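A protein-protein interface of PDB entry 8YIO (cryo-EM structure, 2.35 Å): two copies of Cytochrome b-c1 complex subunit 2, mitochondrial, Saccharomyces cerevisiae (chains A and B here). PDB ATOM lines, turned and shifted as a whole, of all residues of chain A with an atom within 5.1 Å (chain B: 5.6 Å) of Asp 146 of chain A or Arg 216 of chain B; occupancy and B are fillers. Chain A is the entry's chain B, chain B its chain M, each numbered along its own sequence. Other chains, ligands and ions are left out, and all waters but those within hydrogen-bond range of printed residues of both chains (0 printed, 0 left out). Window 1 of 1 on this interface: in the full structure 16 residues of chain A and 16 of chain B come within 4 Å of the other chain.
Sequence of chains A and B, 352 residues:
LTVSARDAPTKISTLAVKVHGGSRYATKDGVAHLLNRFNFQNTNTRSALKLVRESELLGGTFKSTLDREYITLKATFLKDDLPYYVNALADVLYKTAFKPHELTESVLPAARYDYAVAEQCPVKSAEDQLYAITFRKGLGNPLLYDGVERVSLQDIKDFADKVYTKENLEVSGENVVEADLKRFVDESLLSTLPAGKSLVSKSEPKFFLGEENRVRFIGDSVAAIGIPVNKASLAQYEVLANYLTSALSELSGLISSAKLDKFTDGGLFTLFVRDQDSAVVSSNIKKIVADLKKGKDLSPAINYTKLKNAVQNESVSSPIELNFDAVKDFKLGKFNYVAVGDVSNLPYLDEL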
ATOM      1  N   ASP A  29       5.167 -16.122 -16.580  1.00  0.00           N
ATOM      2  CA  ASP A  29       4.975 -16.266 -15.141  1.00  0.00           C
ATOM      3  C   ASP A  29       6.101 -17.092 -14.531  1.00  0.00           C
ATOM      4  O   ASP A  29       6.253 -18.276 -14.848  1.00  0.00           O
ATOM      5  CB  ASP A  29       3.626 -16.918 -14.850  1.00  0.00           C
ATOM      6  CG  ASP A  29       2.466 -15.957 -14.998  1.00  0.00           C
ATOM      7  OD1 ASP A  29       2.700 -14.775 -15.320  1.00  0.00           O
ATOM      8  OD2 ASP A  29       1.315 -16.386 -14.791  1.00  0.00           O
ATOM      9  N   TYR A 115       8.248 -22.682  -3.510  1.00  0.00           N
ATOM     10  CA  TYR A 115       6.811 -22.523  -3.686  1.00  0.00           C
ATOM     11  C   TYR A 115       6.030 -23.266  -2.607  1.00  0.00           C
ATOM     12  O   TYR A 115       4.980 -22.795  -2.162  1.00  0.00           O
ATOM     13  CB  TYR A 115       6.398 -22.999  -5.079  1.00  0.00           C
ATOM     14  CG  TYR A 115       4.920 -22.864  -5.349  1.00  0.00           C
ATOM     15  CD1 TYR A 115       4.359 -21.628  -5.629  1.00  0.00           C
ATOM     16  CD2 TYR A 115       4.082 -23.971  -5.303  1.00  0.00           C
ATOM     17  CE1 TYR A 115       3.009 -21.497  -5.860  1.00  0.00           C
ATOM     18  CE2 TYR A 115       2.733 -23.851  -5.531  1.00  0.00           C
ATOM     19  CZ  TYR A 115       2.202 -22.614  -5.811  1.00  0.00           C
ATOM     20  OH  TYR A 115       0.853 -22.496  -6.044  1.00  0.00           O
ATOM     21  N   PRO A 142       2.668 -12.656 -10.514  1.00  0.00           N
ATOM     22  CA  PRO A 142       3.072 -13.586  -9.456  1.00  0.00           C
ATOM     23  C   PRO A 142       4.582 -13.593  -9.271  1.00  0.00           C
ATOM     24  O   PRO A 142       5.354 -13.464 -10.223  1.00  0.00           O
ATOM     25  CB  PRO A 142       2.566 -14.941  -9.962  1.00  0.00           C
ATOM     26  CG  PRO A 142       2.427 -14.778 -11.424  1.00  0.00           C
ATOM     27  CD  PRO A 142       2.038 -13.354 -11.646  1.00  0.00           C
ATOM     28  N   LEU A 144       6.565 -16.096  -7.556  1.00  0.00           N
ATOM     29  CA  LEU A 144       7.226 -17.388  -7.662  1.00  0.00           C
ATOM     30  C   LEU A 144       6.702 -18.184  -8.853  1.00  0.00           C
ATOM     31  O   LEU A 144       5.682 -17.858  -9.459  1.00  0.00           O
ATOM     32  CB  LEU A 144       7.048 -18.185  -6.368  1.00  0.00           C
ATOM     33  CG  LEU A 144       7.617 -17.578  -5.083  1.00  0.00           C
ATOM     34  CD1 LEU A 144       7.350 -18.491  -3.902  1.00  0.00           C
ATOM     35  CD2 LEU A 144       9.105 -17.295  -5.214  1.00  0.00           C
ATOM     36  N   TYR A 145       7.425 -19.251  -9.176  1.00  0.00           N
ATOM     37  CA  TYR A 145       7.084 -20.137 -10.280  1.00  0.00           C
ATOM     38  C   TYR A 145       6.251 -21.308  -9.770  1.00  0.00           C
ATOM     39  O   TYR A 145       6.655 -22.001  -8.830  1.00  0.00           O
ATOM     40  CB  TYR A 145       8.361 -20.641 -10.958  1.00  0.00           C
ATOM     41  CG  TYR A 145       8.155 -21.685 -12.031  1.00  0.00           C
ATOM     42  CD1 TYR A 145       7.693 -21.332 -13.291  1.00  0.00           C
ATOM     43  CD2 TYR A 145       8.440 -23.021 -11.789  1.00  0.00           C
ATOM     44  CE1 TYR A 145       7.510 -22.282 -14.273  1.00  0.00           C
ATOM     45  CE2 TYR A 145       8.258 -23.975 -12.762  1.00  0.00           C
ATOM     46  CZ  TYR A 145       7.796 -23.599 -14.001  1.00  0.00           C
ATOM     47  OH  TYR A 145       7.616 -24.549 -14.976  1.00  0.00           O
ATOM     48  N   ASP A 146       5.090 -21.531 -10.390  1.00  0.00           N
ATOM     49  CA  ASP A 146       4.228 -22.646 -10.023  1.00  0.00           C
ATOM     50  C   ASP A 146       3.925 -23.600 -11.170  1.00  0.00           C
ATOM     51  O   ASP A 146       3.451 -24.711 -10.912  1.00  0.00           O
ATOM     52  CB  ASP A 146       2.901 -22.141  -9.422  1.00  0.00           C
ATOM     53  CG  ASP A 146       2.224 -21.069 -10.267  1.00  0.00           C
ATOM     54  OD1 ASP A 146       2.679 -20.783 -11.392  1.00  0.00           O
ATOM     55  OD2 ASP A 146       1.220 -20.500  -9.795  1.00  0.00           O
ATOM     56  N   GLY A 147       4.169 -23.207 -12.413  1.00  0.00           N
ATOM     57  CA  GLY A 147       4.023 -24.114 -13.529  1.00  0.00           C
ATOM     58  C   GLY A 147       2.713 -24.059 -14.281  1.00  0.00           C
ATOM     59  O   GLY A 147       2.413 -25.001 -15.020  1.00  0.00           O
ATOM     60  N   VAL A 148       1.920 -22.997 -14.132  1.00  0.00           N
ATOM     61  CA  VAL A 148       0.723 -22.910 -14.962  1.00  0.00           C
ATOM     62  C   VAL A 148       1.087 -22.404 -16.358  1.00  0.00           C
ATOM     63  O   VAL A 148       0.384 -22.697 -17.331  1.00  0.00           O
ATOM     64  CB  VAL A 148      -0.375 -22.055 -14.293  1.00  0.00           C
ATOM     65  CG1 VAL A 148      -0.614 -22.511 -12.864  1.00  0.00           C
ATOM     66  CG2 VAL A 148      -0.063 -20.582 -14.331  1.00  0.00           C
ATOM     67  N   ARG B 214     -11.223 -15.104 -10.217  1.00  0.00           N
ATOM     68  CA  ARG B 214     -10.158 -15.696 -11.028  1.00  0.00           C
ATOM     69  C   ARG B 214      -9.394 -16.727 -10.209  1.00  0.00           C
ATOM     70  O   ARG B 214      -9.011 -16.451  -9.070  1.00  0.00           O
ATOM     71  CB  ARG B 214      -9.175 -14.628 -11.542  1.00  0.00           C
ATOM     72  CG  ARG B 214      -9.807 -13.450 -12.257  1.00  0.00           C
ATOM     73  CD  ARG B 214      -8.792 -12.383 -12.624  1.00  0.00           C
ATOM     74  NE  ARG B 214      -8.053 -12.716 -13.836  1.00  0.00           N
ATOM     75  CZ  ARG B 214      -8.497 -12.502 -15.070  1.00  0.00           C
ATOM     76  NH1 ARG B 214      -7.751 -12.841 -16.105  1.00  0.00           N
ATOM     77  NH2 ARG B 214      -9.684 -11.952 -15.271  1.00  0.00           N
ATOM     78  N   VAL B 215      -9.172 -17.915 -10.786  1.00  0.00           N
ATOM     79  CA  VAL B 215      -8.492 -19.026 -10.117  1.00  0.00           C
ATOM     80  C   VAL B 215      -7.384 -19.552 -11.028  1.00  0.00           C
ATOM     81  O   VAL B 215      -7.619 -19.793 -12.216  1.00  0.00           O
ATOM     82  CB  VAL B 215      -9.459 -20.179  -9.758  1.00  0.00           C
ATOM     83  CG1 VAL B 215      -8.789 -21.176  -8.830  1.00  0.00           C
ATOM     84  CG2 VAL B 215     -10.756 -19.681  -9.131  1.00  0.00           C
ATOM     85  N   ARG B 216      -6.191 -19.762 -10.467  1.00  0.00           N
ATOM     86  CA  ARG B 216      -5.083 -20.364 -11.208  1.00  0.00           C
ATOM     87  C   ARG B 216      -5.174 -21.886 -11.179  1.00  0.00           C
ATOM     88  O   ARG B 216      -5.527 -22.480 -10.158  1.00  0.00           O
ATOM     89  CB  ARG B 216      -3.738 -19.922 -10.628  1.00  0.00           C
ATOM     90  CG  ARG B 216      -3.504 -18.429 -10.665  1.00  0.00           C
ATOM     91  CD  ARG B 216      -2.215 -18.033  -9.956  1.00  0.00           C
ATOM     92  NE  ARG B 216      -1.018 -18.338 -10.736  1.00  0.00           N
ATOM     93  CZ  ARG B 216      -0.545 -17.581 -11.721  1.00  0.00           C
ATOM     94  NH1 ARG B 216       0.551 -17.943 -12.363  1.00  0.00           N
ATOM     95  NH2 ARG B 216      -1.161 -16.462 -12.066  1.00  0.00           N
ATOM     96  N   PHE B 217      -4.832 -22.517 -12.301  1.00  0.00           N
ATOM     97  CA  PHE B 217      -5.051 -23.948 -12.469  1.00  0.00           C
ATOM     98  C   PHE B 217      -4.123 -24.476 -13.557  1.00  0.00           C
ATOM     99  O   PHE B 217      -3.881 -23.792 -14.552  1.00  0.00           O
ATOM    100  CB  PHE B 217      -6.524 -24.222 -12.819  1.00  0.00           C
ATOM    101  CG  PHE B 217      -6.840 -25.665 -13.090  1.00  0.00           C
ATOM    102  CD1 PHE B 217      -6.989 -26.564 -12.047  1.00  0.00           C
ATOM    103  CD2 PHE B 217      -7.008 -26.119 -14.390  1.00  0.00           C
ATOM    104  CE1 PHE B 217      -7.287 -27.891 -12.294  1.00  0.00           C
ATOM    105  CE2 PHE B 217      -7.301 -27.444 -14.645  1.00  0.00           C
ATOM    106  CZ  PHE B 217      -7.443 -28.331 -13.596  1.00  0.00           C
ATOM    107  N   ILE B 218      -3.617 -25.692 -13.366  1.00  0.00           N
ATOM    108  CA  ILE B 218      -2.760 -26.361 -14.341  1.00  0.00           C
ATOM    109  C   ILE B 218      -3.633 -27.274 -15.194  1.00  0.00           C
ATOM    110  O   ILE B 218      -4.147 -28.286 -14.708  1.00  0.00           O
ATOM    111  CB  ILE B 218      -1.636 -27.159 -13.664  1.00  0.00           C
ATOM    112  CG1 ILE B 218      -0.725 -26.242 -12.853  1.00  0.00           C
ATOM    113  CG2 ILE B 218      -0.820 -27.914 -14.701  1.00  0.00           C
ATOM    114  CD1 ILE B 218       0.415 -26.958 -12.175  1.00  0.00           C
ATOM    115  N   ALA B 339     -12.994 -16.952 -14.464  1.00  0.00           N
ATOM    116  CA  ALA B 339     -11.901 -17.394 -15.323  1.00  0.00           C
ATOM    117  C   ALA B 339     -11.032 -18.381 -14.561  1.00  0.00           C
ATOM    118  O   ALA B 339     -10.600 -18.092 -13.444  1.00  0.00           O
ATOM    119  CB  ALA B 339     -11.059 -16.207 -15.807  1.00  0.00           C
ATOM    120  N   GLY B 341      -7.695 -21.134 -14.924  1.00  0.00           N
ATOM    121  CA  GLY B 341      -6.570 -21.629 -15.694  1.00  0.00           C
ATOM    122  C   GLY B 341      -5.393 -20.681 -15.782  1.00  0.00           C
ATOM    123  O   GLY B 341      -4.826 -20.286 -14.763  1.00  0.00           O
ATOM    124  N   VAL B 343      -4.668 -17.437 -16.034  1.00  0.00           N
ATOM    125  CA  VAL B 343      -5.429 -16.199 -15.868  1.00  0.00           C
ATOM    126  C   VAL B 343      -4.656 -14.949 -16.250  1.00  0.00           C
ATOM    127  O   VAL B 343      -5.258 -13.876 -16.362  1.00  0.00           O
ATOM    128  CB  VAL B 343      -5.941 -16.071 -14.421  1.00  0.00           C
ATOM    129  CG1 VAL B 343      -7.037 -17.088 -14.165  1.00  0.00           C
ATOM    130  CG2 VAL B 343      -4.805 -16.253 -13.437  1.00  0.00           C
ATOM    131  N   SER B 344      -3.342 -15.051 -16.466  1.00  0.00           N
ATOM    132  CA  SER B 344      -2.581 -13.913 -16.964  1.00  0.00           C
ATOM    133  C   SER B 344      -2.883 -13.609 -18.425  1.00  0.00           C
ATOM    134  O   SER B 344      -2.638 -12.486 -18.873  1.00  0.00           O
ATOM    135  CB  SER B 344      -1.082 -14.154 -16.790  1.00  0.00           C
ATOM    136  OG  SER B 344      -0.708 -14.088 -15.427  1.00  0.00           O
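Of the 9 printed residues of chain B, 4 touch a printed residue of chain A.
Printed residues of chain B that touch a printed residue of chain A: Arg 216, Phe 217, Ile 218 and Ser 344.
Hydrophobic or aromatic side chains of chain B that line the printed part of chain A: Ile 218.
Of the 8 printed residues of chain A, 5 touch a printed residue of chain B.
The guanidinium group (NH1) of Arg 216 of chain B lies within salt-bridge range of the side-chain carboxylate (OD2) of Asp 29 of chain A, 3.0 Å away.
OD2 of Asp 29 of chain A sits at hydrogen-bond distance from OG of Ser 344 of chain B (3.1 Å).
The side-chain carboxylate (OD2) of Asp 146 of chain A lies within salt-bridge range of the guanidinium group (NE) of Arg 216 of chain B (3.3 Å).
Among the printed residues, merely in contact across the chains: Val 148 of chain A with Arg 216 of chain B, Val 148 of chain A with Ile 218 of chain B, Pro 142 of chain A with Arg 216 of chain B, Val 148 of chain A with Phe 217 of chain B, Asp 146 of chain A with Ile 218 of chain B and Gly 147 of chain A with Ile 218 of chain B.
Of the printed residues of chain B, Pro 142 of chain A touches Arg 216.
Leu 144 of chain A touches none of the printed residues of chain B.
Of the printed residues of chain B, Val 148 of chain A touches Arg 216 (3.3 Å), Phe 217 (3.9 Å) and Ile 218 (3.7 Å).
Of chain A, only Asp 29 (3.0 Å), Pro 142 (3.8 Å), Asp 146 (3.3 Å) and Val 148 (3.3 Å) come within 4 Å of Arg 216 of chain B.
Of the printed residues of chain A, Phe 217 of chain B touches Val 148.
Of the printed residues of chain A, Ile 218 of chain B touches Asp 146, Gly 147 and Val 148.
Printed residues of chain A within 4 Å of Ser 344 of chain B: Asp 29 (3.1 Å).
The nearest printed residue of chain B that does not touch Asp 146 of chain A is Phe 217 of chain B (6.9 Å).
No position is printed for both chains.
Of the 9 pairs that touch across the chains among the printed residues, none has its exchanged pair printed and touching as well.
The backbone NH (N) of Phe 217 of chain B is in hydrogen-bond range of the backbone carbonyl oxygen (O) of Gly 341 of chain B (3.3 Å).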
